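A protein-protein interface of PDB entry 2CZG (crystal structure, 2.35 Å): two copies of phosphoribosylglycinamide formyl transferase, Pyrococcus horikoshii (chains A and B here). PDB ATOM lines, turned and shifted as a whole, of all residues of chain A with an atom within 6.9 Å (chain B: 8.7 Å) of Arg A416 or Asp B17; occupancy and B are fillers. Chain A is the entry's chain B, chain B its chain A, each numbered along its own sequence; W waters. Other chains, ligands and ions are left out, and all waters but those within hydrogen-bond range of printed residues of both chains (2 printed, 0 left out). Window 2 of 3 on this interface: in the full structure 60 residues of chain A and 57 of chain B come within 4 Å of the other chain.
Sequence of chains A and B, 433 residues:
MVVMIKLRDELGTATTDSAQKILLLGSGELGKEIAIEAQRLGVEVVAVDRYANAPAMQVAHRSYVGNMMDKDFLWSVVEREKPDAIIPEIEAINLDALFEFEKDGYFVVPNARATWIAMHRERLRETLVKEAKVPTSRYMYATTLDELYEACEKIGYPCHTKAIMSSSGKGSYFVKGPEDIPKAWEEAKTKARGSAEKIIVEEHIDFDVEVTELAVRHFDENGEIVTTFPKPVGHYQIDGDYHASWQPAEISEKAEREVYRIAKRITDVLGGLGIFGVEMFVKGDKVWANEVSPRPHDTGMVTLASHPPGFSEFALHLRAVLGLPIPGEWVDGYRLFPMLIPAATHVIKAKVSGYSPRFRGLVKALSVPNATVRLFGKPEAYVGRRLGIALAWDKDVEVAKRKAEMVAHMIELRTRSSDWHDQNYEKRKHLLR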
ATOM      1  N   SER A 353     -13.824  18.996 -15.880  1.00  0.00           N
ATOM      2  CA  SER A 353     -13.610  20.254 -16.568  1.00  0.00           C
ATOM      3  C   SER A 353     -14.480  20.284 -17.820  1.00  0.00           C
ATOM      4  O   SER A 353     -15.136  19.296 -18.169  1.00  0.00           O
ATOM      5  CB  SER A 353     -12.136  20.399 -16.963  1.00  0.00           C
ATOM      6  OG  SER A 353     -11.821  19.530 -18.040  1.00  0.00           O
ATOM      7  N   GLY A 354     -14.488  21.420 -18.502  1.00  0.00           N
ATOM      8  CA  GLY A 354     -15.286  21.504 -19.705  1.00  0.00           C
ATOM      9  C   GLY A 354     -16.334  22.603 -19.729  1.00  0.00           C
ATOM     10  O   GLY A 354     -16.684  23.218 -18.709  1.00  0.00           O
ATOM     11  N   TYR A 355     -16.853  22.818 -20.928  1.00  0.00           N
ATOM     12  CA  TYR A 355     -17.842  23.845 -21.202  1.00  0.00           C
ATOM     13  C   TYR A 355     -19.287  23.350 -21.084  1.00  0.00           C
ATOM     14  O   TYR A 355     -19.559  22.157 -21.219  1.00  0.00           O
ATOM     15  CB  TYR A 355     -17.589  24.371 -22.617  1.00  0.00           C
ATOM     16  CG  TYR A 355     -17.568  25.871 -22.726  1.00  0.00           C
ATOM     17  CD1 TYR A 355     -18.746  26.579 -22.938  1.00  0.00           C
ATOM     18  CD2 TYR A 355     -16.379  26.591 -22.571  1.00  0.00           C
ATOM     19  CE1 TYR A 355     -18.756  27.960 -22.992  1.00  0.00           C
ATOM     20  CE2 TYR A 355     -16.376  27.990 -22.626  1.00  0.00           C
ATOM     21  CZ  TYR A 355     -17.576  28.663 -22.836  1.00  0.00           C
ATOM     22  OH  TYR A 355     -17.623  30.037 -22.881  1.00  0.00           O
ATOM     23  N   SER A 356     -20.204  24.278 -20.817  1.00  0.00           N
ATOM     24  CA  SER A 356     -21.635  23.976 -20.748  1.00  0.00           C
ATOM     25  C   SER A 356     -22.025  22.957 -19.691  1.00  0.00           C
ATOM     26  O   SER A 356     -22.569  21.900 -20.021  1.00  0.00           O
ATOM     27  CB  SER A 356     -22.116  23.464 -22.123  1.00  0.00           C
ATOM     28  OG  SER A 356     -21.663  24.309 -23.174  1.00  0.00           O
ATOM     29  N   PRO A 357     -21.789  23.270 -18.405  1.00  0.00           N
ATOM     30  CA  PRO A 357     -22.134  22.343 -17.321  1.00  0.00           C
ATOM     31  C   PRO A 357     -23.644  22.056 -17.242  1.00  0.00           C
ATOM     32  O   PRO A 357     -24.475  22.854 -17.683  1.00  0.00           O
ATOM     33  CB  PRO A 357     -21.634  23.077 -16.053  1.00  0.00           C
ATOM     34  CG  PRO A 357     -20.601  24.085 -16.575  1.00  0.00           C
ATOM     35  CD  PRO A 357     -21.250  24.536 -17.870  1.00  0.00           C
ATOM     36  N   ARG A 358     -23.994  20.910 -16.676  1.00  0.00           N
ATOM     37  CA  ARG A 358     -25.386  20.541 -16.497  1.00  0.00           C
ATOM     38  C   ARG A 358     -25.493  19.703 -15.236  1.00  0.00           C
ATOM     39  O   ARG A 358     -24.533  19.058 -14.829  1.00  0.00           O
ATOM     40  CB  ARG A 358     -25.961  19.821 -17.742  1.00  0.00           C
ATOM     41  CG  ARG A 358     -25.246  18.611 -18.259  1.00  0.00           C
ATOM     42  CD  ARG A 358     -26.036  18.008 -19.437  1.00  0.00           C
ATOM     43  NE  ARG A 358     -25.845  18.729 -20.689  1.00  0.00           N
ATOM     44  CZ  ARG A 358     -26.694  18.709 -21.718  1.00  0.00           C
ATOM     45  NH1 ARG A 358     -27.819  18.012 -21.647  1.00  0.00           N
ATOM     46  NH2 ARG A 358     -26.406  19.355 -22.845  1.00  0.00           N
ATOM     47  N   ARG A 414     -22.100  17.213 -15.039  1.00  0.00           N
ATOM     48  CA  ARG A 414     -21.597  16.784 -16.326  1.00  0.00           C
ATOM     49  C   ARG A 414     -21.174  18.038 -17.086  1.00  0.00           C
ATOM     50  O   ARG A 414     -21.647  19.134 -16.819  1.00  0.00           O
ATOM     51  CB  ARG A 414     -22.710  16.076 -17.104  1.00  0.00           C
ATOM     52  CG  ARG A 414     -22.242  14.950 -17.967  1.00  0.00           C
ATOM     53  CD  ARG A 414     -22.362  15.297 -19.414  1.00  0.00           C
ATOM     54  NE  ARG A 414     -23.697  15.106 -19.962  1.00  0.00           N
ATOM     55  CZ  ARG A 414     -24.047  15.549 -21.168  1.00  0.00           C
ATOM     56  NH1 ARG A 414     -23.160  16.199 -21.911  1.00  0.00           N
ATOM     57  NH2 ARG A 414     -25.261  15.333 -21.645  1.00  0.00           N
ATOM     58  N   THR A 415     -20.291  17.848 -18.046  1.00  0.00           N
ATOM     59  CA  THR A 415     -19.790  18.914 -18.882  1.00  0.00           C
ATOM     60  C   THR A 415     -19.997  18.408 -20.315  1.00  0.00           C
ATOM     61  O   THR A 415     -20.299  17.235 -20.505  1.00  0.00           O
ATOM     62  CB  THR A 415     -18.308  19.135 -18.543  1.00  0.00           C
ATOM     63  OG1 THR A 415     -18.181  20.299 -17.705  1.00  0.00           O
ATOM     64  CG2 THR A 415     -17.481  19.248 -19.776  1.00  0.00           C
ATOM     65  N   ARG A 416     -19.877  19.282 -21.308  1.00  0.00           N
ATOM     66  CA  ARG A 416     -20.051  18.909 -22.715  1.00  0.00           C
ATOM     67  C   ARG A 416     -19.150  17.748 -23.092  1.00  0.00           C
ATOM     68  O   ARG A 416     -19.484  16.945 -23.958  1.00  0.00           O
ATOM     69  CB  ARG A 416     -19.664  20.060 -23.652  1.00  0.00           C
ATOM     70  CG  ARG A 416     -20.764  20.969 -24.106  1.00  0.00           C
ATOM     71  CD  ARG A 416     -20.236  21.857 -25.236  1.00  0.00           C
ATOM     72  NE  ARG A 416     -19.862  21.020 -26.363  1.00  0.00           N
ATOM     73  CZ  ARG A 416     -20.719  20.509 -27.240  1.00  0.00           C
ATOM     74  NH1 ARG A 416     -22.022  20.757 -27.149  1.00  0.00           N
ATOM     75  NH2 ARG A 416     -20.272  19.696 -28.180  1.00  0.00           N
ATOM     76  N   SER A 417     -17.988  17.684 -22.457  1.00  0.00           N
ATOM     77  CA  SER A 417     -17.028  16.652 -22.782  1.00  0.00           C
ATOM     78  C   SER A 417     -16.649  15.750 -21.614  1.00  0.00           C
ATOM     79  O   SER A 417     -15.508  15.303 -21.537  1.00  0.00           O
ATOM     80  CB  SER A 417     -15.766  17.311 -23.328  1.00  0.00           C
ATOM     81  OG  SER A 417     -15.189  18.130 -22.320  1.00  0.00           O
ATOM     82  N   SER A 418     -17.583  15.481 -20.708  1.00  0.00           N
ATOM     83  CA  SER A 418     -17.266  14.618 -19.573  1.00  0.00           C
ATOM     84  C   SER A 418     -18.429  13.710 -19.218  1.00  0.00           C
ATOM     85  O   SER A 418     -19.523  13.833 -19.762  1.00  0.00           O
ATOM     86  CB  SER A 418     -16.889  15.452 -18.334  1.00  0.00           C
ATOM     87  OG  SER A 418     -18.035  15.768 -17.540  1.00  0.00           O
ATOM     88  N   GLU B  10     -33.060  17.530 -14.760  1.00  0.00           N
ATOM     89  CA  GLU B  10     -31.814  18.181 -15.163  1.00  0.00           C
ATOM     90  C   GLU B  10     -31.949  19.624 -15.666  1.00  0.00           C
ATOM     91  O   GLU B  10     -32.999  20.024 -16.178  1.00  0.00           O
ATOM     92  CB  GLU B  10     -31.171  17.314 -16.270  1.00  0.00           C
ATOM     93  CG  GLU B  10     -29.831  17.790 -16.852  1.00  0.00           C
ATOM     94  CD  GLU B  10     -29.962  18.775 -18.020  1.00  0.00           C
ATOM     95  OE1 GLU B  10     -31.089  19.038 -18.479  1.00  0.00           O
ATOM     96  OE2 GLU B  10     -28.921  19.285 -18.491  1.00  0.00           O
ATOM     97  N   GLY B  12     -29.273  22.784 -17.591  1.00  0.00           N
ATOM     98  CA  GLY B  12     -27.989  23.133 -18.157  1.00  0.00           C
ATOM     99  C   GLY B  12     -27.617  24.524 -17.658  1.00  0.00           C
ATOM    100  O   GLY B  12     -28.184  25.009 -16.671  1.00  0.00           O
ATOM    101  N   THR B  13     -26.705  25.175 -18.373  1.00  0.00           N
ATOM    102  CA  THR B  13     -26.198  26.499 -18.011  1.00  0.00           C
ATOM    103  C   THR B  13     -26.478  27.602 -19.043  1.00  0.00           C
ATOM    104  O   THR B  13     -26.158  27.467 -20.233  1.00  0.00           O
ATOM    105  CB  THR B  13     -24.664  26.424 -17.791  1.00  0.00           C
ATOM    106  OG1 THR B  13     -24.377  25.411 -16.814  1.00  0.00           O
ATOM    107  CG2 THR B  13     -24.113  27.756 -17.330  1.00  0.00           C
ATOM    108  N   ALA B  14     -27.059  28.700 -18.569  1.00  0.00           N
ATOM    109  CA  ALA B  14     -27.369  29.868 -19.404  1.00  0.00           C
ATOM    110  C   ALA B  14     -26.111  30.404 -20.105  1.00  0.00           C
ATOM    111  O   ALA B  14     -25.018  30.436 -19.517  1.00  0.00           O
ATOM    112  CB  ALA B  14     -27.989  30.983 -18.534  1.00  0.00           C
ATOM    113  N   THR B  15     -26.298  30.846 -21.349  1.00  0.00           N
ATOM    114  CA  THR B  15     -25.253  31.389 -22.229  1.00  0.00           C
ATOM    115  C   THR B  15     -24.419  30.303 -22.894  1.00  0.00           C
ATOM    116  O   THR B  15     -23.537  30.627 -23.697  1.00  0.00           O
ATOM    117  CB  THR B  15     -24.271  32.442 -21.537  1.00  0.00           C
ATOM    118  OG1 THR B  15     -23.275  31.770 -20.751  1.00  0.00           O
ATOM    119  CG2 THR B  15     -25.055  33.439 -20.658  1.00  0.00           C
ATOM    120  N   THR B  16     -24.683  29.034 -22.552  1.00  0.00           N
ATOM    121  CA  THR B  16     -23.986  27.884 -23.179  1.00  0.00           C
ATOM    122  C   THR B  16     -25.022  27.064 -23.962  1.00  0.00           C
ATOM    123  O   THR B  16     -26.225  27.344 -23.885  1.00  0.00           O
ATOM    124  CB  THR B  16     -23.319  26.920 -22.163  1.00  0.00           C
ATOM    125  OG1 THR B  16     -24.316  26.082 -21.562  1.00  0.00           O
ATOM    126  CG2 THR B  16     -22.571  27.707 -21.069  1.00  0.00           C
ATOM    127  N   ASP B  17     -24.576  26.041 -24.689  1.00  0.00           N
ATOM    128  CA  ASP B  17     -25.516  25.255 -25.480  1.00  0.00           C
ATOM    129  C   ASP B  17     -26.366  24.282 -24.667  1.00  0.00           C
ATOM    130  O   ASP B  17     -27.307  23.711 -25.194  1.00  0.00           O
ATOM    131  CB  ASP B  17     -24.795  24.494 -26.605  1.00  0.00           C
ATOM    132  CG  ASP B  17     -23.891  23.401 -26.074  1.00  0.00           C
ATOM    133  OD1 ASP B  17     -24.139  22.222 -26.392  1.00  0.00           O
ATOM    134  OD2 ASP B  17     -22.936  23.720 -25.342  1.00  0.00           O
ATOM    135  N   SER B  18     -26.064  24.105 -23.384  1.00  0.00           N
ATOM    136  CA  SER B  18     -26.863  23.189 -22.573  1.00  0.00           C
ATOM    137  C   SER B  18     -27.982  23.935 -21.859  1.00  0.00           C
ATOM    138  O   SER B  18     -28.738  23.340 -21.080  1.00  0.00           O
ATOM    139  CB  SER B  18     -25.982  22.473 -21.534  1.00  0.00           C
ATOM    140  OG  SER B  18     -25.527  23.353 -20.497  1.00  0.00           O
ATOM    141  N   ALA B  19     -28.109  25.229 -22.148  1.00  0.00           N
ATOM    142  CA  ALA B  19     -29.103  26.081 -21.483  1.00  0.00           C
ATOM    143  C   ALA B  19     -30.578  25.814 -21.711  1.00  0.00           C
ATOM    144  O   ALA B  19     -30.972  25.398 -22.796  1.00  0.00           O
ATOM    145  CB  ALA B  19     -28.835  27.559 -21.825  1.00  0.00           C
ATOM    146  N   GLN B  20     -31.379  26.046 -20.664  1.00  0.00           N
ATOM    147  CA  GLN B  20     -32.827  25.974 -20.787  1.00  0.00           C
ATOM    148  C   GLN B  20     -33.127  27.446 -20.949  1.00  0.00           C
ATOM    149  O   GLN B  20     -32.362  28.287 -20.480  1.00  0.00           O
ATOM    150  CB  GLN B  20     -33.527  25.479 -19.524  1.00  0.00           C
ATOM    151  CG  GLN B  20     -33.730  23.985 -19.508  1.00  0.00           C
ATOM    152  CD  GLN B  20     -32.415  23.275 -19.432  1.00  0.00           C
ATOM    153  OE1 GLN B  20     -31.665  23.459 -18.481  1.00  0.00           O
ATOM    154  NE2 GLN B  20     -32.117  22.462 -20.427  1.00  0.00           N
ATOM    155  N   GLU B  44     -31.482  30.534 -18.914  1.00  0.00           N
ATOM    156  CA  GLU B  44     -31.415  31.671 -19.822  1.00  0.00           C
ATOM    157  C   GLU B  44     -32.767  32.397 -19.898  1.00  0.00           C
ATOM    158  O   GLU B  44     -33.817  31.773 -19.982  1.00  0.00           O
ATOM    159  CB  GLU B  44     -30.980  31.195 -21.205  1.00  0.00           C
ATOM    160  CG  GLU B  44     -30.493  32.289 -22.139  1.00  0.00           C
ATOM    161  CD  GLU B  44     -29.530  31.740 -23.163  1.00  0.00           C
ATOM    162  OE1 GLU B  44     -29.692  32.055 -24.360  1.00  0.00           O
ATOM    163  OE2 GLU B  44     -28.603  30.993 -22.771  1.00  0.00           O
ATOM    164  N   ASP B  84     -38.033  26.863 -23.882  1.00  0.00           N
ATOM    165  CA  ASP B  84     -38.615  25.734 -23.173  1.00  0.00           C
ATOM    166  C   ASP B  84     -39.976  26.131 -22.610  1.00  0.00           C
ATOM    167  O   ASP B  84     -40.832  25.283 -22.395  1.00  0.00           O
ATOM    168  CB  ASP B  84     -37.685  25.269 -22.037  1.00  0.00           C
ATOM    169  CG  ASP B  84     -36.386  24.683 -22.569  1.00  0.00           C
ATOM    170  OD1 ASP B  84     -35.399  25.432 -22.752  1.00  0.00           O
ATOM    171  OD2 ASP B  84     -36.371  23.473 -22.849  1.00  0.00           O
HETATM  172  O   HOH W   1     -24.048  20.562 -24.291  1.00  0.00           O
HETATM  173  O   HOH W   2     -29.542  20.776 -20.889  1.00  0.00           O
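The side-chain carboxylate (OE2) of Glu B10 is in salt-bridge range of the guanidinium group (NH1) of Arg A358 (3.6 Å). The side-chain hydroxyl of Thr B13 is in hydrogen-bond range of the backbone carbonyl oxygen of Pro A357 (2.7 Å). The side-chain hydroxyl (OG) of Ser A356 sits at hydrogen-bond distance from the side-chain carboxylate (OD2) of Asp B17 (2.6 Å). The guanidinium group (NH1) of Arg A416 lies within salt-bridge range of the side-chain carboxylate (OD1) of Asp B17 (2.7 Å). O of Ser A356 is in hydrogen-bond range of OG of Ser B18 (3.3 Å). The backbone carbonyl oxygen of Pro A357 is in hydrogen-bond range of the side-chain hydroxyl of Ser B18, at 3.0 Å.
The side-chain amide oxygen (OE1) of Gln B20 sits at hydrogen-bond distance from the backbone NH (N) of Gly B12. The backbone carbonyl oxygen (O) of Thr B13 lies within hydrogen-bond range of the side-chain hydroxyl (OG1) of Thr B16, at 2.7 Å. N of Thr B13 is in hydrogen-bond range of OG of Ser B18, at 3.0 Å. OG1 of Thr B16 sits at hydrogen-bond distance from OG of Ser B18 (3.2 Å). The backbone NH (N) of Arg A416 lies within hydrogen-bond range of the backbone carbonyl oxygen (O) of Tyr A355 (2.9 Å). O of Arg A414 is in hydrogen-bond range of N of Arg A358 (2.9 Å).
OG of Ser A356 touches CB of Thr B16, 3.3 Å away. O of Pro A357 touches CA of Gly B12, at 3.6 Å. CB of Arg A358 touches CA of Gly B12, at 3.9 Å. CB of Ser B18 touches NH2 of Arg A358, at 3.4 Å.
Ser A353 touches none of the printed residues of chain B. Of the printed residues of chain B, Ser A356 touches Thr B16 (3.3 Å), Asp B17 (2.6 Å) and Ser B18 (3.3 Å). No residue of chain B comes within 4 Å of Thr A415. Printed residues of chain B within 4 Å of Arg A416: Asp B17 (2.7 Å). Of the printed residues of chain A, Glu B10 touches Arg A358 (3.1 Å). Of the printed residues of chain A, Gly B12 touches Pro A357 and Arg A358. Printed residues of chain A within 4 Å of Thr B13: Pro A357. Of the printed residues of chain A, Thr B16 touches Ser A356 (3.3 Å). Of chain A, only Ser A356 and Arg A416 come within 4 Å of Asp B17. The nearest residue of chain B that does not touch Arg A416 is Ser B18 (6.0 Å). The nearest residue of chain A that does not touch Asp B17 is Arg A358 (5.0 Å).
Hydrophobic or aromatic side chains of chain A within 4 Å of the printed part of chain B: Pro A357.
No position is printed for both chains. Of the 10 pairs that touch across the chains among the printed residues, none has its exchanged pair printed and touching as well.
Water W1 lies within hydrogen-bond range of OD1 of Asp B17 (2.7 Å) and NH2 of Arg A358 (3.0 Å). Water W2 lies within hydrogen-bond range of the backbone carbonyl oxygen of Ser B18 (2.7 Å), the side-chain carboxylate of Glu B10 (2.9 Å), the side-chain amide nitrogen of Gln B20 (3.1 Å) and the guanidinium group of Arg A358 (3.3 Å).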
